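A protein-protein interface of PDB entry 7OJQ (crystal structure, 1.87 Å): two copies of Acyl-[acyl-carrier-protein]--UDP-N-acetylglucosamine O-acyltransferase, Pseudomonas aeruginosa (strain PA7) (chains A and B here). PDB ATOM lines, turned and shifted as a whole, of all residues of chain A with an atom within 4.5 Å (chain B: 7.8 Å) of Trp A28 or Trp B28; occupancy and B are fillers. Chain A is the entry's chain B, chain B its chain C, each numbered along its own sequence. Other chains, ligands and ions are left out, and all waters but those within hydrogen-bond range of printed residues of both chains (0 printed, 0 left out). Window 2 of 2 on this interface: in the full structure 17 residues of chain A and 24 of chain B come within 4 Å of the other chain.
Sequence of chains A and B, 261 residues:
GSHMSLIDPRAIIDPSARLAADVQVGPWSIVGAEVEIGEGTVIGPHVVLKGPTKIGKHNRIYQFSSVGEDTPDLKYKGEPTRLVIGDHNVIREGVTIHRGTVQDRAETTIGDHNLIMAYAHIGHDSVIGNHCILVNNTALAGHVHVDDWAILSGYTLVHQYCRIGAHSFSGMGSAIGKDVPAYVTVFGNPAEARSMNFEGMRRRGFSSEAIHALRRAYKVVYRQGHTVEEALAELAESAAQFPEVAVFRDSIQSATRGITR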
ATOM      1  N   ARG A  10      20.370  19.193  23.845  1.00  0.00           N
ATOM      2  CA  ARG A  10      19.042  19.185  23.216  1.00  0.00           C
ATOM      3  C   ARG A  10      18.040  20.120  23.909  1.00  0.00           C
ATOM      4  O   ARG A  10      16.909  20.263  23.451  1.00  0.00           O
ATOM      5  CB  ARG A  10      18.475  17.763  23.078  1.00  0.00           C
ATOM      6  CG  ARG A  10      19.247  16.908  22.080  1.00  0.00           C
ATOM      7  CD  ARG A  10      19.126  15.433  22.371  1.00  0.00           C
ATOM      8  NE  ARG A  10      19.743  15.104  23.661  1.00  0.00           N
ATOM      9  CZ  ARG A  10      20.065  13.877  24.049  1.00  0.00           C
ATOM     10  NH1 ARG A  10      19.891  12.847  23.227  1.00  0.00           N
ATOM     11  NH2 ARG A  10      20.588  13.671  25.253  1.00  0.00           N
ATOM     12  N   ALA A  11      18.444  20.726  25.028  1.00  0.00           N
ATOM     13  CA  ALA A  11      17.605  21.690  25.734  1.00  0.00           C
ATOM     14  C   ALA A  11      17.793  23.061  25.055  1.00  0.00           C
ATOM     15  O   ALA A  11      18.808  23.280  24.383  1.00  0.00           O
ATOM     16  CB  ALA A  11      18.027  21.763  27.204  1.00  0.00           C
ATOM     17  N   GLY A  26      17.629  18.536  31.610  1.00  0.00           N
ATOM     18  CA  GLY A  26      17.401  17.371  30.762  1.00  0.00           C
ATOM     19  C   GLY A  26      17.121  17.734  29.308  1.00  0.00           C
ATOM     20  O   GLY A  26      16.914  18.909  28.973  1.00  0.00           O
ATOM     21  N   PRO A  27      17.072  16.718  28.417  1.00  0.00           N
ATOM     22  CA  PRO A  27      16.846  16.994  26.991  1.00  0.00           C
ATOM     23  C   PRO A  27      15.436  17.540  26.700  1.00  0.00           C
ATOM     24  O   PRO A  27      14.487  17.232  27.426  1.00  0.00           O
ATOM     25  CB  PRO A  27      17.086  15.625  26.337  1.00  0.00           C
ATOM     26  CG  PRO A  27      16.761  14.639  27.412  1.00  0.00           C
ATOM     27  CD  PRO A  27      17.296  15.277  28.655  1.00  0.00           C
ATOM     28  N   TRP A  28      15.320  18.365  25.641  1.00  0.00           N
ATOM     29  CA  TRP A  28      14.075  18.982  25.155  1.00  0.00           C
ATOM     30  C   TRP A  28      13.380  19.857  26.202  1.00  0.00           C
ATOM     31  O   TRP A  28      12.150  19.982  26.205  1.00  0.00           O
ATOM     32  CB  TRP A  28      13.123  17.927  24.571  1.00  0.00           C
ATOM     33  CG  TRP A  28      13.841  16.852  23.808  1.00  0.00           C
ATOM     34  CD1 TRP A  28      14.554  16.998  22.653  1.00  0.00           C
ATOM     35  CD2 TRP A  28      14.006  15.491  24.216  1.00  0.00           C
ATOM     36  NE1 TRP A  28      15.114  15.797  22.289  1.00  0.00           N
ATOM     37  CE2 TRP A  28      14.790  14.850  23.230  1.00  0.00           C
ATOM     38  CE3 TRP A  28      13.523  14.735  25.299  1.00  0.00           C
ATOM     39  CZ2 TRP A  28      15.109  13.486  23.294  1.00  0.00           C
ATOM     40  CZ3 TRP A  28      13.833  13.380  25.356  1.00  0.00           C
ATOM     41  CH2 TRP A  28      14.633  12.779  24.385  1.00  0.00           C
ATOM     42  N   SER A  29      14.168  20.453  27.112  1.00  0.00           N
ATOM     43  CA  SER A  29      13.584  21.375  28.083  1.00  0.00           C
ATOM     44  C   SER A  29      13.823  22.777  27.583  1.00  0.00           C
ATOM     45  O   SER A  29      14.751  22.991  26.805  1.00  0.00           O
ATOM     46  CB  SER A  29      14.147  21.163  29.479  1.00  0.00           C
ATOM     47  OG  SER A  29      13.559  19.996  30.019  1.00  0.00           O
ATOM     48  N   ILE A  30      12.961  23.714  27.976  1.00  0.00           N
ATOM     49  CA  ILE A  30      13.084  25.113  27.588  1.00  0.00           C
ATOM     50  C   ILE A  30      13.274  25.934  28.833  1.00  0.00           C
ATOM     51  O   ILE A  30      12.432  25.898  29.735  1.00  0.00           O
ATOM     52  CB  ILE A  30      11.848  25.628  26.769  1.00  0.00           C
ATOM     53  CG1 ILE A  30      11.607  24.767  25.510  1.00  0.00           C
ATOM     54  CG2 ILE A  30      11.984  27.137  26.444  1.00  0.00           C
ATOM     55  CD1 ILE A  30      10.252  25.004  24.728  1.00  0.00           C
ATOM     56  N   HIS A  46      11.800  17.625  28.941  1.00  0.00           N
ATOM     57  CA  HIS A  46      10.450  18.103  28.561  1.00  0.00           C
ATOM     58  C   HIS A  46       9.856  19.093  29.587  1.00  0.00           C
ATOM     59  O   HIS A  46       8.683  18.983  29.953  1.00  0.00           O
ATOM     60  CB  HIS A  46       9.483  16.903  28.426  1.00  0.00           C
ATOM     61  CG  HIS A  46       9.896  15.845  27.463  1.00  0.00           C
ATOM     62  ND1 HIS A  46       9.951  16.088  26.103  1.00  0.00           N
ATOM     63  CD2 HIS A  46      10.174  14.541  27.687  1.00  0.00           C
ATOM     64  CE1 HIS A  46      10.270  14.935  25.548  1.00  0.00           C
ATOM     65  NE2 HIS A  46      10.401  13.972  26.464  1.00  0.00           N
ATOM     66  N   VAL A  47      10.671  19.989  30.122  1.00  0.00           N
ATOM     67  CA  VAL A  47      10.169  20.952  31.112  1.00  0.00           C
ATOM     68  C   VAL A  47      10.087  22.276  30.416  1.00  0.00           C
ATOM     69  O   VAL A  47      11.001  22.619  29.673  1.00  0.00           O
ATOM     70  CB  VAL A  47      11.035  21.038  32.409  1.00  0.00           C
ATOM     71  CG1 VAL A  47      10.618  22.233  33.301  1.00  0.00           C
ATOM     72  CG2 VAL A  47      10.987  19.745  33.203  1.00  0.00           C
ATOM     73  N   ASP B   8      12.988   5.508  16.650  1.00  0.00           N
ATOM     74  CA  ASP B   8      13.218   6.805  16.037  1.00  0.00           C
ATOM     75  C   ASP B   8      14.635   7.297  16.436  1.00  0.00           C
ATOM     76  O   ASP B   8      15.003   7.142  17.587  1.00  0.00           O
ATOM     77  CB  ASP B   8      12.118   7.810  16.459  1.00  0.00           C
ATOM     78  CG  ASP B   8      12.208   9.116  15.707  1.00  0.00           C
ATOM     79  OD1 ASP B   8      13.096   9.927  16.039  1.00  0.00           O
ATOM     80  OD2 ASP B   8      11.421   9.311  14.762  1.00  0.00           O
ATOM     81  N   PRO B   9      15.455   7.852  15.507  1.00  0.00           N
ATOM     82  CA  PRO B   9      16.800   8.337  15.898  1.00  0.00           C
ATOM     83  C   PRO B   9      16.821   9.501  16.918  1.00  0.00           C
ATOM     84  O   PRO B   9      17.878   9.820  17.481  1.00  0.00           O
ATOM     85  CB  PRO B   9      17.448   8.717  14.551  1.00  0.00           C
ATOM     86  CG  PRO B   9      16.323   8.987  13.665  1.00  0.00           C
ATOM     87  CD  PRO B   9      15.188   8.100  14.079  1.00  0.00           C
ATOM     88  N   ARG B  10      15.660  10.109  17.190  1.00  0.00           N
ATOM     89  CA  ARG B  10      15.549  11.195  18.184  1.00  0.00           C
ATOM     90  C   ARG B  10      15.214  10.682  19.594  1.00  0.00           C
ATOM     91  O   ARG B  10      15.185  11.465  20.541  1.00  0.00           O
ATOM     92  CB  ARG B  10      14.532  12.250  17.723  1.00  0.00           C
ATOM     93  CG  ARG B  10      15.019  13.036  16.522  1.00  0.00           C
ATOM     94  CD  ARG B  10      13.863  13.614  15.732  1.00  0.00           C
ATOM     95  NE  ARG B  10      13.052  12.575  15.091  1.00  0.00           N
ATOM     96  CZ  ARG B  10      12.273  12.785  14.035  1.00  0.00           C
ATOM     97  NH1 ARG B  10      12.222  13.982  13.469  1.00  0.00           N
ATOM     98  NH2 ARG B  10      11.541  11.797  13.534  1.00  0.00           N
ATOM     99  N   ALA B  11      14.954   9.381  19.726  1.00  0.00           N
ATOM    100  CA  ALA B  11      14.667   8.735  21.000  1.00  0.00           C
ATOM    101  C   ALA B  11      16.004   8.407  21.708  1.00  0.00           C
ATOM    102  O   ALA B  11      17.050   8.314  21.063  1.00  0.00           O
ATOM    103  CB  ALA B  11      13.892   7.447  20.755  1.00  0.00           C
ATOM    104  N   ILE B  12      15.951   8.254  23.040  1.00  0.00           N
ATOM    105  CA  ILE B  12      17.097   7.900  23.873  1.00  0.00           C
ATOM    106  C   ILE B  12      16.864   6.512  24.449  1.00  0.00           C
ATOM    107  O   ILE B  12      15.922   6.310  25.213  1.00  0.00           O
ATOM    108  CB  ILE B  12      17.374   8.941  24.983  1.00  0.00           C
ATOM    109  CG1 ILE B  12      17.648  10.348  24.397  1.00  0.00           C
ATOM    110  CG2 ILE B  12      18.555   8.457  25.873  1.00  0.00           C
ATOM    111  CD1 ILE B  12      17.774  11.455  25.490  1.00  0.00           C
ATOM    112  N   VAL B  25       9.749   2.824  18.932  1.00  0.00           N
ATOM    113  CA  VAL B  25       9.901   3.911  19.915  1.00  0.00           C
ATOM    114  C   VAL B  25       9.864   5.219  19.139  1.00  0.00           C
ATOM    115  O   VAL B  25      10.687   5.427  18.238  1.00  0.00           O
ATOM    116  CB  VAL B  25      11.164   3.796  20.816  1.00  0.00           C
ATOM    117  CG1 VAL B  25      11.249   4.978  21.787  1.00  0.00           C
ATOM    118  CG2 VAL B  25      11.186   2.476  21.602  1.00  0.00           C
ATOM    119  N   GLY B  26       8.911   6.071  19.489  1.00  0.00           N
ATOM    120  CA  GLY B  26       8.702   7.354  18.825  1.00  0.00           C
ATOM    121  C   GLY B  26       9.735   8.412  19.165  1.00  0.00           C
ATOM    122  O   GLY B  26      10.546   8.211  20.067  1.00  0.00           O
ATOM    123  N   PRO B  27       9.735   9.561  18.450  1.00  0.00           N
ATOM    124  CA  PRO B  27      10.744  10.609  18.736  1.00  0.00           C
ATOM    125  C   PRO B  27      10.633  11.215  20.136  1.00  0.00           C
ATOM    126  O   PRO B  27       9.537  11.264  20.680  1.00  0.00           O
ATOM    127  CB  PRO B  27      10.440  11.685  17.683  1.00  0.00           C
ATOM    128  CG  PRO B  27       9.004  11.459  17.309  1.00  0.00           C
ATOM    129  CD  PRO B  27       8.829   9.972  17.354  1.00  0.00           C
ATOM    130  N   TRP B  28      11.778  11.689  20.694  1.00  0.00           N
ATOM    131  CA  TRP B  28      11.895  12.371  21.998  1.00  0.00           C
ATOM    132  C   TRP B  28      11.385  11.525  23.163  1.00  0.00           C
ATOM    133  O   TRP B  28      10.869  12.048  24.136  1.00  0.00           O
ATOM    134  CB  TRP B  28      11.198  13.756  21.950  1.00  0.00           C
ATOM    135  CG  TRP B  28      11.449  14.459  20.657  1.00  0.00           C
ATOM    136  CD1 TRP B  28      12.658  14.843  20.153  1.00  0.00           C
ATOM    137  CD2 TRP B  28      10.473  14.810  19.672  1.00  0.00           C
ATOM    138  NE1 TRP B  28      12.489  15.442  18.927  1.00  0.00           N
ATOM    139  CE2 TRP B  28      11.159  15.412  18.594  1.00  0.00           C
ATOM    140  CE3 TRP B  28       9.081  14.625  19.572  1.00  0.00           C
ATOM    141  CZ2 TRP B  28      10.502  15.866  17.442  1.00  0.00           C
ATOM    142  CZ3 TRP B  28       8.421  15.109  18.447  1.00  0.00           C
ATOM    143  CH2 TRP B  28       9.132  15.696  17.385  1.00  0.00           C
ATOM    144  N   SER B  29      11.486  10.210  23.034  1.00  0.00           N
ATOM    145  CA  SER B  29      11.052   9.341  24.106  1.00  0.00           C
ATOM    146  C   SER B  29      12.299   8.823  24.802  1.00  0.00           C
ATOM    147  O   SER B  29      13.344   8.721  24.167  1.00  0.00           O
ATOM    148  CB  SER B  29      10.235   8.184  23.561  1.00  0.00           C
ATOM    149  OG  SER B  29       8.922   8.651  23.325  1.00  0.00           O
ATOM    150  N   ILE B  30      12.196   8.539  26.106  1.00  0.00           N
ATOM    151  CA  ILE B  30      13.311   8.010  26.870  1.00  0.00           C
ATOM    152  C   ILE B  30      12.968   6.612  27.355  1.00  0.00           C
ATOM    153  O   ILE B  30      11.979   6.426  28.069  1.00  0.00           O
ATOM    154  CB  ILE B  30      13.731   8.946  28.035  1.00  0.00           C
ATOM    155  CG1 ILE B  30      14.217  10.305  27.492  1.00  0.00           C
ATOM    156  CG2 ILE B  30      14.825   8.274  28.924  1.00  0.00           C
ATOM    157  CD1 ILE B  30      14.285  11.469  28.543  1.00  0.00           C
ATOM    158  N   VAL B  31      13.807   5.639  26.985  1.00  0.00           N
ATOM    159  CA  VAL B  31      13.691   4.276  27.482  1.00  0.00           C
ATOM    160  C   VAL B  31      14.881   4.164  28.440  1.00  0.00           C
ATOM    161  O   VAL B  31      16.028   4.099  28.006  1.00  0.00           O
ATOM    162  CB  VAL B  31      13.665   3.216  26.363  1.00  0.00           C
ATOM    163  CG1 VAL B  31      13.705   1.802  26.942  1.00  0.00           C
ATOM    164  CG2 VAL B  31      12.442   3.408  25.468  1.00  0.00           C
ATOM    165  N   GLY B  44       5.003   5.530  22.071  1.00  0.00           N
ATOM    166  CA  GLY B  44       4.697   6.740  21.313  1.00  0.00           C
ATOM    167  C   GLY B  44       5.788   7.781  21.473  1.00  0.00           C
ATOM    168  O   GLY B  44       6.842   7.497  22.049  1.00  0.00           O
ATOM    169  N   PRO B  45       5.577   9.003  20.954  1.00  0.00           N
ATOM    170  CA  PRO B  45       6.589  10.056  21.154  1.00  0.00           C
ATOM    171  C   PRO B  45       6.457  10.672  22.557  1.00  0.00           C
ATOM    172  O   PRO B  45       5.426  10.495  23.208  1.00  0.00           O
ATOM    173  CB  PRO B  45       6.209  11.087  20.094  1.00  0.00           C
ATOM    174  CG  PRO B  45       4.676  10.982  20.006  1.00  0.00           C
ATOM    175  CD  PRO B  45       4.366   9.521  20.251  1.00  0.00           C
ATOM    176  N   HIS B  46       7.480  11.439  23.022  1.00  0.00           N
ATOM    177  CA  HIS B  46       7.418  12.130  24.331  1.00  0.00           C
ATOM    178  C   HIS B  46       7.067  11.226  25.540  1.00  0.00           C
ATOM    179  O   HIS B  46       6.338  11.652  26.443  1.00  0.00           O
ATOM    180  CB  HIS B  46       6.425  13.305  24.303  1.00  0.00           C
ATOM    181  CG  HIS B  46       6.708  14.323  23.269  1.00  0.00           C
ATOM    182  ND1 HIS B  46       7.857  15.073  23.309  1.00  0.00           N
ATOM    183  CD2 HIS B  46       5.967  14.707  22.214  1.00  0.00           C
ATOM    184  CE1 HIS B  46       7.793  15.883  22.270  1.00  0.00           C
ATOM    185  NE2 HIS B  46       6.678  15.694  21.580  1.00  0.00           N
ATOM    186  N   VAL B  47       7.521   9.985  25.527  1.00  0.00           N
ATOM    187  CA  VAL B  47       7.218   9.059  26.617  1.00  0.00           C
ATOM    188  C   VAL B  47       8.443   8.924  27.523  1.00  0.00           C
ATOM    189  O   VAL B  47       9.551   8.853  27.018  1.00  0.00           O
ATOM    190  CB  VAL B  47       6.781   7.672  26.046  1.00  0.00           C
ATOM    191  CG1 VAL B  47       6.617   6.634  27.172  1.00  0.00           C
ATOM    192  CG2 VAL B  47       5.486   7.802  25.230  1.00  0.00           C
ATOM    193  N   VAL B  48       8.252   8.876  28.855  1.00  0.00           N
ATOM    194  CA  VAL B  48       9.373   8.632  29.766  1.00  0.00           C
ATOM    195  C   VAL B  48       9.168   7.272  30.417  1.00  0.00           C
ATOM    196  O   VAL B  48       8.134   7.040  31.055  1.00  0.00           O
ATOM    197  CB  VAL B  48       9.565   9.769  30.800  1.00  0.00           C
ATOM    198  CG1 VAL B  48      10.657   9.424  31.826  1.00  0.00           C
ATOM    199  CG2 VAL B  48       9.878  11.081  30.095  1.00  0.00           C
ATOM    200  N   PHE B  64       3.493  11.711  26.692  1.00  0.00           N
ATOM    201  CA  PHE B  64       3.459  12.436  27.972  1.00  0.00           C
ATOM    202  C   PHE B  64       3.185  11.535  29.189  1.00  0.00           C
ATOM    203  O   PHE B  64       2.960  12.039  30.272  1.00  0.00           O
ATOM    204  CB  PHE B  64       2.479  13.659  27.915  1.00  0.00           C
ATOM    205  CG  PHE B  64       2.569  14.416  26.608  1.00  0.00           C
ATOM    206  CD1 PHE B  64       3.793  14.875  26.132  1.00  0.00           C
ATOM    207  CD2 PHE B  64       1.429  14.667  25.850  1.00  0.00           C
ATOM    208  CE1 PHE B  64       3.873  15.569  24.916  1.00  0.00           C
ATOM    209  CE2 PHE B  64       1.514  15.353  24.635  1.00  0.00           C
ATOM    210  CZ  PHE B  64       2.735  15.811  24.187  1.00  0.00           C
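NE2 of His A46 is in hydrogen-bond range of O of Trp B28 (3.1 Å).
The guanidinium group of Arg B10 lies within salt-bridge range of the side-chain carboxylate of Asp B8 (2.8 Å). O of Arg B10 is in hydrogen-bond range of N of Trp B28, 3.4 Å away. The backbone NH (N) of Val B31 is in hydrogen-bond range of the backbone carbonyl oxygen (O) of Ile B12. The backbone NH of His B46 lies within hydrogen-bond range of the backbone carbonyl oxygen of Pro B27. O of Val B47 lies within hydrogen-bond range of N of Ile B30, 2.8 Å away. O of His B46 sits at hydrogen-bond distance from N of Phe B64.
Arg A10 touches Ile B12 (NH1 to CD1, 3.4 Å). CD1 of Ile B12 touches CG of Pro A27 (3.9 Å). Trp A28 touches Arg B10. CD1 of Ile B12 touches CH2 of Trp A28, at 3.6 Å. Trp A28 touches Trp B28 (NE1 to CD1, 3.4 Å). Trp A28 touches Ile B30 (CZ3 to CD1, 3.7 Å). His A46 touches His B46 (CE1 to ND1, 3.3 Å).
Of chain B, only Arg B10, Ile B12, Trp B28 and Ile B30 come within 4 Å of Trp A28. Of chain A, only Trp A28 and His A46 come within 4 Å of Trp B28. Printed residues of chain A within 4 Å of Ile B30: Trp A28 (3.7 Å). Of the printed residues of chain B, His A46 touches Trp B28 (3.1 Å) and His B46 (3.3 Å). Of the printed residues of chain B, Pro A27 touches Ile B12. Of the printed residues of chain A, Ile B12 touches Arg A10, Pro A27 and Trp A28. Of the printed residues of chain A, His B46 touches His A46 (3.3 Å). Phe B64 touches none of the printed residues of chain A. The nearest residue of chain B that does not touch Trp A28 is Ser B29 (4.3 Å). The nearest printed residue of chain B that does not touch Pro A27 is Ile B30 (4.2 Å).
Of the 9 printed residues of chain A, 4 touch a printed residue of chain B. Printed residues of chain A that touch a printed residue of chain B: Arg A10, Pro A27, Trp A28 and His A46. Hydrophobic or aromatic side chains of chain A within 4 Å of the printed part of chain B: Pro A27, Trp A28 and His A46. Along chain A the printed residues that touch a printed residue of chain B span positions 10 to 46. Of the 18 printed residues of chain B, 5 touch a printed residue of chain A. Among the printed residues, no Asp or Glu carboxylate lies within 4 Å of a Lys or Arg side-chain nitrogen of the other chain.
Trp A28 touches its own counterpart, Trp B28. Trp A28 touches Ile B30, but with the chains exchanged Ile A30 does not touch Trp B28 (11.3 Å). His A46 touches Trp B28, but with the chains exchanged Trp A28 does not touch His B46 (6.0 Å). His A46 touches its own counterpart, His B46. Of the 8 pairs that touch across the chains among the printed residues, 2 have their exchanged pair printed and touching as well.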
